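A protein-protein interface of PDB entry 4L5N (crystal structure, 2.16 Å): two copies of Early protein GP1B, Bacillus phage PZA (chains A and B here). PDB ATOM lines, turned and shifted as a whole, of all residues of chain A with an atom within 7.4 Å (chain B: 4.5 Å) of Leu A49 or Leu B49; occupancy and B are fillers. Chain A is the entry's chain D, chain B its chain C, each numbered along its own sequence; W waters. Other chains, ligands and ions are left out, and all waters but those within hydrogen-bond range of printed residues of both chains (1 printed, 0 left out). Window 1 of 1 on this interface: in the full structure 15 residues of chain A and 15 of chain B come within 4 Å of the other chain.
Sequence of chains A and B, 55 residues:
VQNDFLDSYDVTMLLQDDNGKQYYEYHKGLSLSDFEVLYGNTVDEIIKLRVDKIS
Leu A49 touches its own counterpart, Leu B49. Leu A49 touches Arg B50, and with the chains exchanged Arg A50 touches Leu B49. Leu A49 touches Val B51, and with the chains exchanged Val A51 touches Leu B49. Arg B50 touches its own counterpart, Arg A50. Positions printed for both chains: 11, 12, 13, 35, 46, 48, 49, 50 and 51. Of the 13 pairs that touch across the chains among the printed residues, 8 have their exchanged pair printed and touching as well.
N of Thr A12 sits at hydrogen-bond distance from O of Arg A50 (2.9 Å). N of Asp A52 sits at hydrogen-bond distance from O of Asp A10 (2.9 Å). N of Arg B50 is in hydrogen-bond range of O of Thr B12 (2.9 Å). N of Leu A14 is in hydrogen-bond range of O of Lys A48 (3.0 Å).
CD2 of Phe B35 touches OH of Tyr A39, at 3.9 Å. CA of Lys A48 touches O of Val B51, 3.3 Å away. O of Leu A49 touches O of Leu B49, at 3.9 Å. Leu A49 touches Arg B50. Arg A50 touches Leu B49. NH1 of Arg B50 touches CG of Arg A50, at 3.4 Å. Val A51 touches Lys B48. O of Val A51 touches NH1 of Arg B50, 3.999 Å away. CG of Lys B48 touches OD1 of Asp A52 (3.4 Å).
The backbone carbonyl oxygen (O) of Leu A49 sits at hydrogen-bond distance from the backbone NH (N) of Val B51, at 2.8 Å. OH of Tyr A9 lies within hydrogen-bond range of O of Ile B46 (2.8 Å). The backbone NH (N) of Leu B49 sits at hydrogen-bond distance from the backbone carbonyl oxygen (O) of Val A51. The guanidinium group (NH1) of Arg B50 is in salt-bridge range of the side-chain carboxylate (OD1) of Asp A52 (2.6 Å).
Water W1 bridges NZ of Lys B48 and O of Lys A53.
Printed residues of chain B within 4 Å of Tyr A9: Ile B46. Asp A10 touches none of the printed residues of chain B. Printed residues of chain B within 4 Å of Tyr A39: Phe B35. Printed residues of chain B within 4 Å of Leu A49: Leu B49 (3.9 Å), Arg B50 (3.4 Å) and Val B51 (2.8 Å). Printed residues of chain B within 4 Å of Arg A50: Leu B49 and Arg B50. Val B11 touches none of the printed residues of chain A. Of the printed residues of chain A, Phe B35 touches Tyr A39 (3.9 Å). Of the printed residues of chain A, Lys B48 touches Val A51 (3.4 Å) and Asp A52 (3.4 Å). Of chain A, only Leu A49 (3.9 Å), Arg A50 (3.3 Å) and Val A51 (2.8 Å) come within 4 Å of Leu B49. The nearest printed residue of chain B that does not touch Leu A49 is Phe B35 (4.2 Å). The nearest residue of chain A that does not touch Leu B49 is Asp A52 (4.1 Å).
Hydrophobic or aromatic side chains of chain A within 4 Å of the printed part of chain B: Tyr A9, Tyr A39, Leu A49 and Val A51. Hydrophobic or aromatic side chains of chain B that line the printed part of chain A: Phe B35, Leu B49 and Val B51.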
ATOM      1  N   TYR A   9     -13.381 -12.313 -11.105  1.00  0.00           N
ATOM      2  CA  TYR A   9     -13.370 -12.073 -12.533  1.00  0.00           C
ATOM      3  C   TYR A   9     -12.030 -11.625 -13.062  1.00  0.00           C
ATOM      4  O   TYR A   9     -11.258 -10.990 -12.350  1.00  0.00           O
ATOM      5  CB  TYR A   9     -14.385 -10.937 -12.827  1.00  0.00           C
ATOM      6  CG  TYR A   9     -15.823 -11.303 -12.558  1.00  0.00           C
ATOM      7  CD1 TYR A   9     -16.392 -11.106 -11.300  1.00  0.00           C
ATOM      8  CD2 TYR A   9     -16.635 -11.798 -13.574  1.00  0.00           C
ATOM      9  CE1 TYR A   9     -17.720 -11.447 -11.050  1.00  0.00           C
ATOM     10  CE2 TYR A   9     -17.962 -12.148 -13.335  1.00  0.00           C
ATOM     11  CZ  TYR A   9     -18.503 -11.965 -12.076  1.00  0.00           C
ATOM     12  OH  TYR A   9     -19.818 -12.298 -11.872  1.00  0.00           O
ATOM     13  N   ASP A  10     -11.788 -11.908 -14.330  1.00  0.00           N
ATOM     14  CA  ASP A  10     -10.655 -11.391 -15.083  1.00  0.00           C
ATOM     15  C   ASP A  10     -11.291 -10.235 -15.849  1.00  0.00           C
ATOM     16  O   ASP A  10     -12.314 -10.431 -16.506  1.00  0.00           O
ATOM     17  CB  ASP A  10     -10.119 -12.431 -16.076  1.00  0.00           C
ATOM     18  CG  ASP A  10      -9.091 -13.381 -15.479  1.00  0.00           C
ATOM     19  OD1 ASP A  10      -8.697 -13.173 -14.331  1.00  0.00           O
ATOM     20  OD2 ASP A  10      -8.704 -14.335 -16.163  1.00  0.00           O
ATOM     21  N   VAL A  11     -10.749  -9.025 -15.675  1.00  0.00           N
ATOM     22  CA  VAL A  11     -11.235  -7.802 -16.314  1.00  0.00           C
ATOM     23  C   VAL A  11     -10.117  -7.274 -17.245  1.00  0.00           C
ATOM     24  O   VAL A  11      -8.977  -7.075 -16.811  1.00  0.00           O
ATOM     25  CB  VAL A  11     -11.706  -6.712 -15.295  1.00  0.00           C
ATOM     26  CG1 VAL A  11     -12.242  -5.474 -16.040  1.00  0.00           C
ATOM     27  CG2 VAL A  11     -12.784  -7.265 -14.353  1.00  0.00           C
ATOM     28  N   THR A  12     -10.466  -7.062 -18.506  1.00  0.00           N
ATOM     29  CA  THR A  12      -9.578  -6.553 -19.541  1.00  0.00           C
ATOM     30  C   THR A  12     -10.224  -5.306 -20.119  1.00  0.00           C
ATOM     31  O   THR A  12     -11.429  -5.304 -20.385  1.00  0.00           O
ATOM     32  CB  THR A  12      -9.358  -7.639 -20.617  1.00  0.00           C
ATOM     33  OG1 THR A  12      -8.673  -8.721 -20.008  1.00  0.00           O
ATOM     34  CG2 THR A  12      -8.538  -7.148 -21.842  1.00  0.00           C
ATOM     35  N   MET A  13      -9.419  -4.260 -20.325  1.00  0.00           N
ATOM     36  CA  MET A  13      -9.875  -3.036 -20.975  1.00  0.00           C
ATOM     37  C   MET A  13      -8.895  -2.638 -22.032  1.00  0.00           C
ATOM     38  O   MET A  13      -7.687  -2.743 -21.820  1.00  0.00           O
ATOM     39  CB  MET A  13     -10.025  -1.872 -19.970  1.00  0.00           C
ATOM     40  CG  MET A  13     -11.391  -1.856 -19.258  1.00  0.00           C
ATOM     41  SD  MET A  13     -11.662  -0.554 -17.984  1.00  0.00           S
ATOM     42  CE  MET A  13     -10.345  -0.881 -16.954  1.00  0.00           C
ATOM     43  N   LEU A  14      -9.418  -2.190 -23.184  1.00  0.00           N
ATOM     44  CA  LEU A  14      -8.661  -1.564 -24.241  1.00  0.00           C
ATOM     45  C   LEU A  14      -9.126  -0.111 -24.154  1.00  0.00           C
ATOM     46  O   LEU A  14     -10.319   0.181 -24.309  1.00  0.00           O
ATOM     47  CB  LEU A  14      -8.946  -2.165 -25.623  1.00  0.00           C
ATOM     48  CG  LEU A  14      -8.267  -1.474 -26.831  1.00  0.00           C
ATOM     49  CD1 LEU A  14      -6.742  -1.530 -26.733  1.00  0.00           C
ATOM     50  CD2 LEU A  14      -8.712  -2.104 -28.144  1.00  0.00           C
ATOM     51  N   LEU A  32     -17.278  -8.213  -8.474  1.00  0.00           N
ATOM     52  CA  LEU A  32     -18.052  -7.277  -9.308  1.00  0.00           C
ATOM     53  C   LEU A  32     -18.017  -5.869  -8.714  1.00  0.00           C
ATOM     54  O   LEU A  32     -18.079  -4.904  -9.467  1.00  0.00           O
ATOM     55  CB  LEU A  32     -19.523  -7.711  -9.535  1.00  0.00           C
ATOM     56  CG  LEU A  32     -19.908  -8.436 -10.836  1.00  0.00           C
ATOM     57  CD1 LEU A  32     -21.415  -8.404 -11.037  1.00  0.00           C
ATOM     58  CD2 LEU A  32     -19.226  -7.862 -12.054  1.00  0.00           C
ATOM     59  N   PHE A  35     -14.862  -4.302  -9.907  1.00  0.00           N
ATOM     60  CA  PHE A  35     -15.051  -3.890 -11.303  1.00  0.00           C
ATOM     61  C   PHE A  35     -15.787  -2.540 -11.412  1.00  0.00           C
ATOM     62  O   PHE A  35     -15.436  -1.716 -12.263  1.00  0.00           O
ATOM     63  CB  PHE A  35     -15.761  -4.992 -12.134  1.00  0.00           C
ATOM     64  CG  PHE A  35     -16.433  -4.451 -13.370  1.00  0.00           C
ATOM     65  CD1 PHE A  35     -15.683  -4.049 -14.469  1.00  0.00           C
ATOM     66  CD2 PHE A  35     -17.816  -4.294 -13.417  1.00  0.00           C
ATOM     67  CE1 PHE A  35     -16.306  -3.488 -15.590  1.00  0.00           C
ATOM     68  CE2 PHE A  35     -18.438  -3.746 -14.538  1.00  0.00           C
ATOM     69  CZ  PHE A  35     -17.680  -3.335 -15.611  1.00  0.00           C
ATOM     70  N   LEU A  38     -13.509   0.205 -10.416  1.00  0.00           N
ATOM     71  CA  LEU A  38     -12.551   0.300 -11.531  1.00  0.00           C
ATOM     72  C   LEU A  38     -13.172   1.082 -12.718  1.00  0.00           C
ATOM     73  O   LEU A  38     -12.594   2.064 -13.206  1.00  0.00           O
ATOM     74  CB  LEU A  38     -12.102  -1.093 -11.985  1.00  0.00           C
ATOM     75  CG  LEU A  38     -11.217  -1.154 -13.255  1.00  0.00           C
ATOM     76  CD1 LEU A  38      -9.781  -0.664 -12.974  1.00  0.00           C
ATOM     77  CD2 LEU A  38     -11.177  -2.561 -13.809  1.00  0.00           C
ATOM     78  N   TYR A  39     -14.374   0.671 -13.135  1.00  0.00           N
ATOM     79  CA  TYR A  39     -15.086   1.321 -14.237  1.00  0.00           C
ATOM     80  C   TYR A  39     -15.366   2.823 -13.916  1.00  0.00           C
ATOM     81  O   TYR A  39     -15.026   3.698 -14.718  1.00  0.00           O
ATOM     82  CB  TYR A  39     -16.375   0.540 -14.558  1.00  0.00           C
ATOM     83  CG  TYR A  39     -17.134   1.106 -15.737  1.00  0.00           C
ATOM     84  CD1 TYR A  39     -16.911   0.631 -17.027  1.00  0.00           C
ATOM     85  CD2 TYR A  39     -18.039   2.154 -15.571  1.00  0.00           C
ATOM     86  CE1 TYR A  39     -17.626   1.133 -18.115  1.00  0.00           C
ATOM     87  CE2 TYR A  39     -18.742   2.678 -16.655  1.00  0.00           C
ATOM     88  CZ  TYR A  39     -18.509   2.181 -17.928  1.00  0.00           C
ATOM     89  OH  TYR A  39     -19.164   2.707 -18.994  1.00  0.00           O
ATOM     90  N   ILE A  46     -13.208   4.259 -23.394  1.00  0.00           N
ATOM     91  CA  ILE A  46     -13.348   2.809 -23.475  1.00  0.00           C
ATOM     92  C   ILE A  46     -13.549   2.329 -24.916  1.00  0.00           C
ATOM     93  O   ILE A  46     -14.535   2.700 -25.567  1.00  0.00           O
ATOM     94  CB  ILE A  46     -14.396   2.238 -22.474  1.00  0.00           C
ATOM     95  CG1 ILE A  46     -13.915   2.477 -21.015  1.00  0.00           C
ATOM     96  CG2 ILE A  46     -14.646   0.714 -22.718  1.00  0.00           C
ATOM     97  CD1 ILE A  46     -14.972   2.296 -19.996  1.00  0.00           C
ATOM     98  N   ILE A  47     -12.606   1.483 -25.398  1.00  0.00           N
ATOM     99  CA  ILE A  47     -12.656   0.849 -26.728  1.00  0.00           C
ATOM    100  C   ILE A  47     -13.229  -0.557 -26.568  1.00  0.00           C
ATOM    101  O   ILE A  47     -14.155  -0.920 -27.292  1.00  0.00           O
ATOM    102  CB  ILE A  47     -11.290   0.882 -27.490  1.00  0.00           C
ATOM    103  CG1 ILE A  47     -10.632   2.297 -27.452  1.00  0.00           C
ATOM    104  CG2 ILE A  47     -11.444   0.362 -28.939  1.00  0.00           C
ATOM    105  CD1 ILE A  47     -11.592   3.548 -27.961  1.00  0.00           C
ATOM    106  N   LYS A  48     -12.711  -1.328 -25.589  1.00  0.00           N
ATOM    107  CA  LYS A  48     -13.226  -2.662 -25.261  1.00  0.00           C
ATOM    108  C   LYS A  48     -13.285  -2.845 -23.768  1.00  0.00           C
ATOM    109  O   LYS A  48     -12.442  -2.315 -23.037  1.00  0.00           O
ATOM    110  CB  LYS A  48     -12.342  -3.807 -25.777  1.00  0.00           C
ATOM    111  CG  LYS A  48     -12.115  -3.914 -27.274  1.00  0.00           C
ATOM    112  CD  LYS A  48     -11.087  -5.026 -27.547  1.00  0.00           C
ATOM    113  CE  LYS A  48     -11.543  -6.449 -27.225  1.00  0.00           C
ATOM    114  NZ  LYS A  48     -12.638  -6.912 -28.145  1.00  0.00           N
ATOM    115  N   LEU A  49     -14.246  -3.666 -23.339  1.00  0.00           N
ATOM    116  CA  LEU A  49     -14.386  -4.147 -21.982  1.00  0.00           C
ATOM    117  C   LEU A  49     -14.717  -5.638 -22.063  1.00  0.00           C
ATOM    118  O   LEU A  49     -15.542  -6.041 -22.873  1.00  0.00           O
ATOM    119  CB  LEU A  49     -15.447  -3.357 -21.199  1.00  0.00           C
ATOM    120  CG  LEU A  49     -15.830  -3.911 -19.829  1.00  0.00           C
ATOM    121  CD1 LEU A  49     -14.583  -4.007 -18.867  1.00  0.00           C
ATOM    122  CD2 LEU A  49     -16.948  -3.061 -19.209  1.00  0.00           C
ATOM    123  N   ARG A  50     -13.989  -6.457 -21.289  1.00  0.00           N
ATOM    124  CA  ARG A  50     -14.192  -7.893 -21.179  1.00  0.00           C
ATOM    125  C   ARG A  50     -14.162  -8.242 -19.680  1.00  0.00           C
ATOM    126  O   ARG A  50     -13.201  -7.916 -18.977  1.00  0.00           O
ATOM    127  CB  ARG A  50     -13.088  -8.619 -21.959  1.00  0.00           C
ATOM    128  CG  ARG A  50     -13.276 -10.114 -22.122  1.00  0.00           C
ATOM    129  CD  ARG A  50     -12.499 -10.618 -23.330  1.00  0.00           C
ATOM    130  NE  ARG A  50     -11.070 -10.696 -23.038  1.00  0.00           N
ATOM    131  CZ  ARG A  50     -10.112 -10.145 -23.775  1.00  0.00           C
ATOM    132  NH1 ARG A  50     -10.415  -9.484 -24.885  1.00  0.00           N
ATOM    133  NH2 ARG A  50      -8.843 -10.262 -23.412  1.00  0.00           N
ATOM    134  N   VAL A  51     -15.244  -8.829 -19.177  1.00  0.00           N
ATOM    135  CA  VAL A  51     -15.360  -9.243 -17.775  1.00  0.00           C
ATOM    136  C   VAL A  51     -15.731 -10.722 -17.836  1.00  0.00           C
ATOM    137  O   VAL A  51     -16.732 -11.038 -18.456  1.00  0.00           O
ATOM    138  CB  VAL A  51     -16.403  -8.393 -16.983  1.00  0.00           C
ATOM    139  CG1 VAL A  51     -16.518  -8.867 -15.537  1.00  0.00           C
ATOM    140  CG2 VAL A  51     -16.056  -6.895 -17.012  1.00  0.00           C
ATOM    141  N   ASP A  52     -14.883 -11.634 -17.314  1.00  0.00           N
ATOM    142  CA  ASP A  52     -15.158 -13.089 -17.354  1.00  0.00           C
ATOM    143  C   ASP A  52     -15.010 -13.759 -16.013  1.00  0.00           C
ATOM    144  O   ASP A  52     -13.938 -13.665 -15.410  1.00  0.00           O
ATOM    145  CB  ASP A  52     -14.235 -13.809 -18.362  1.00  0.00           C
ATOM    146  CG  ASP A  52     -14.505 -13.447 -19.812  1.00  0.00           C
ATOM    147  OD1 ASP A  52     -15.606 -12.949 -20.106  1.00  0.00           O
ATOM    148  OD2 ASP A  52     -13.611 -13.621 -20.630  1.00  0.00           O
ATOM    149  N   LYS A  53     -16.044 -14.515 -15.586  1.00  0.00           N
ATOM    150  CA  LYS A  53     -16.014 -15.261 -14.322  1.00  0.00           C
ATOM    151  C   LYS A  53     -14.916 -16.331 -14.402  1.00  0.00           C
ATOM    152  O   LYS A  53     -14.859 -17.063 -15.397  1.00  0.00           O
ATOM    153  CB  LYS A  53     -17.381 -15.892 -14.006  1.00  0.00           C
ATOM    154  CG  LYS A  53     -17.431 -16.553 -12.612  1.00  0.00           C
ATOM    155  CD  LYS A  53     -18.661 -17.429 -12.478  1.00  0.00           C
ATOM    156  CE  LYS A  53     -18.618 -18.297 -11.235  1.00  0.00           C
ATOM    157  NZ  LYS A  53     -19.917 -19.020 -11.034  1.00  0.00           N
ATOM    158  N   VAL B  11     -23.117  -4.729 -26.807  1.00  0.00           N
ATOM    159  CA  VAL B  11     -22.968  -5.377 -25.480  1.00  0.00           C
ATOM    160  C   VAL B  11     -23.483  -6.824 -25.558  1.00  0.00           C
ATOM    161  O   VAL B  11     -24.608  -7.066 -26.000  1.00  0.00           O
ATOM    162  CB  VAL B  11     -23.691  -4.583 -24.332  1.00  0.00           C
ATOM    163  CG1 VAL B  11     -23.458  -5.213 -22.958  1.00  0.00           C
ATOM    164  CG2 VAL B  11     -23.289  -3.113 -24.321  1.00  0.00           C
ATOM    165  N   THR B  12     -22.638  -7.776 -25.179  1.00  0.00           N
ATOM    166  CA  THR B  12     -22.978  -9.193 -25.128  1.00  0.00           C
ATOM    167  C   THR B  12     -22.786  -9.642 -23.679  1.00  0.00           C
ATOM    168  O   THR B  12     -21.780  -9.303 -23.047  1.00  0.00           O
ATOM    169  CB  THR B  12     -22.120 -10.003 -26.112  1.00  0.00           C
ATOM    170  OG1 THR B  12     -22.403  -9.556 -27.446  1.00  0.00           O
ATOM    171  CG2 THR B  12     -22.365 -11.521 -26.010  1.00  0.00           C
ATOM    172  N   MET B  13     -23.764 -10.384 -23.155  1.00  0.00           N
ATOM    173  CA  MET B  13     -23.687 -10.950 -21.820  1.00  0.00           C
ATOM    174  C   MET B  13     -24.042 -12.433 -21.876  1.00  0.00           C
ATOM    175  O   MET B  13     -24.932 -12.835 -22.632  1.00  0.00           O
ATOM    176  CB  MET B  13     -24.658 -10.239 -20.856  1.00  0.00           C
ATOM    177  CG  MET B  13     -24.240  -8.820 -20.493  1.00  0.00           C
ATOM    178  SD  MET B  13     -25.188  -8.073 -19.117  1.00  0.00           S
ATOM    179  CE  MET B  13     -26.674  -7.678 -19.957  1.00  0.00           C
ATOM    180  N   PHE B  35     -25.348   1.503 -21.745  1.00  0.00           N
ATOM    181  CA  PHE B  35     -24.705   0.298 -21.183  1.00  0.00           C
ATOM    182  C   PHE B  35     -24.735   0.365 -19.647  1.00  0.00           C
ATOM    183  O   PHE B  35     -25.069  -0.625 -18.986  1.00  0.00           O
ATOM    184  CB  PHE B  35     -23.246   0.088 -21.704  1.00  0.00           C
ATOM    185  CG  PHE B  35     -22.434  -0.831 -20.798  1.00  0.00           C
ATOM    186  CD1 PHE B  35     -22.793  -2.172 -20.632  1.00  0.00           C
ATOM    187  CD2 PHE B  35     -21.385  -0.328 -20.031  1.00  0.00           C
ATOM    188  CE1 PHE B  35     -22.136  -2.975 -19.687  1.00  0.00           C
ATOM    189  CE2 PHE B  35     -20.679  -1.154 -19.150  1.00  0.00           C
ATOM    190  CZ  PHE B  35     -21.073  -2.460 -18.960  1.00  0.00           C
ATOM    191  N   ILE B  46     -23.602 -12.666 -13.699  1.00  0.00           N
ATOM    192  CA  ILE B  46     -22.787 -12.417 -14.900  1.00  0.00           C
ATOM    193  C   ILE B  46     -21.706 -13.485 -14.998  1.00  0.00           C
ATOM    194  O   ILE B  46     -20.911 -13.658 -14.064  1.00  0.00           O
ATOM    195  CB  ILE B  46     -22.188 -10.964 -14.911  1.00  0.00           C
ATOM    196  CG1 ILE B  46     -23.306  -9.913 -15.147  1.00  0.00           C
ATOM    197  CG2 ILE B  46     -21.043 -10.812 -15.981  1.00  0.00           C
ATOM    198  CD1 ILE B  46     -22.943  -8.447 -14.820  1.00  0.00           C
ATOM    199  N   LYS B  48     -20.053 -13.834 -18.351  1.00  0.00           N
ATOM    200  CA  LYS B  48     -19.242 -13.112 -19.320  1.00  0.00           C
ATOM    201  C   LYS B  48     -19.920 -11.807 -19.675  1.00  0.00           C
ATOM    202  O   LYS B  48     -21.144 -11.754 -19.754  1.00  0.00           O
ATOM    203  CB  LYS B  48     -19.028 -13.943 -20.605  1.00  0.00           C
ATOM    204  CG  LYS B  48     -18.138 -15.148 -20.397  1.00  0.00           C
ATOM    205  CD  LYS B  48     -17.920 -15.961 -21.650  1.00  0.00           C
ATOM    206  CE  LYS B  48     -17.373 -17.337 -21.311  1.00  0.00           C
ATOM    207  NZ  LYS B  48     -16.138 -17.291 -20.463  1.00  0.00           N
ATOM    208  N   LEU B  49     -19.122 -10.760 -19.884  1.00  0.00           N
ATOM    209  CA  LEU B  49     -19.571  -9.440 -20.324  1.00  0.00           C
ATOM    210  C   LEU B  49     -18.541  -8.938 -21.343  1.00  0.00           C
ATOM    211  O   LEU B  49     -17.332  -9.005 -21.090  1.00  0.00           O
ATOM    212  CB  LEU B  49     -19.740  -8.458 -19.131  1.00  0.00           C
ATOM    213  CG  LEU B  49     -19.959  -6.961 -19.425  1.00  0.00           C
ATOM    214  CD1 LEU B  49     -21.342  -6.696 -20.068  1.00  0.00           C
ATOM    215  CD2 LEU B  49     -19.901  -6.141 -18.140  1.00  0.00           C
ATOM    216  N   ARG B  50     -19.049  -8.490 -22.496  1.00  0.00           N
ATOM    217  CA  ARG B  50     -18.271  -7.936 -23.600  1.00  0.00           C
ATOM    218  C   ARG B  50     -18.877  -6.564 -23.956  1.00  0.00           C
ATOM    219  O   ARG B  50     -20.089  -6.460 -24.160  1.00  0.00           O
ATOM    220  CB  ARG B  50     -18.321  -8.854 -24.851  1.00  0.00           C
ATOM    221  CG  ARG B  50     -17.816 -10.295 -24.677  1.00  0.00           C
ATOM    222  CD  ARG B  50     -16.299 -10.374 -24.758  1.00  0.00           C
ATOM    223  NE  ARG B  50     -15.742 -11.723 -24.591  1.00  0.00           N
ATOM    224  CZ  ARG B  50     -15.689 -12.375 -23.434  1.00  0.00           C
ATOM    225  NH1 ARG B  50     -16.231 -11.850 -22.340  1.00  0.00           N
ATOM    226  NH2 ARG B  50     -15.114 -13.568 -23.367  1.00  0.00           N
ATOM    227  N   VAL B  51     -18.039  -5.504 -24.017  1.00  0.00           N
ATOM    228  CA  VAL B  51     -18.496  -4.153 -24.406  1.00  0.00           C
ATOM    229  C   VAL B  51     -17.529  -3.681 -25.499  1.00  0.00           C
ATOM    230  O   VAL B  51     -16.333  -3.644 -25.236  1.00  0.00           O
ATOM    231  CB  VAL B  51     -18.657  -3.111 -23.254  1.00  0.00           C
ATOM    232  CG1 VAL B  51     -19.173  -1.774 -23.805  1.00  0.00           C
ATOM    233  CG2 VAL B  51     -19.605  -3.625 -22.169  1.00  0.00           C
HETATM  234  O   HOH W   1     -16.293 -17.050 -17.762  1.00  0.00           O
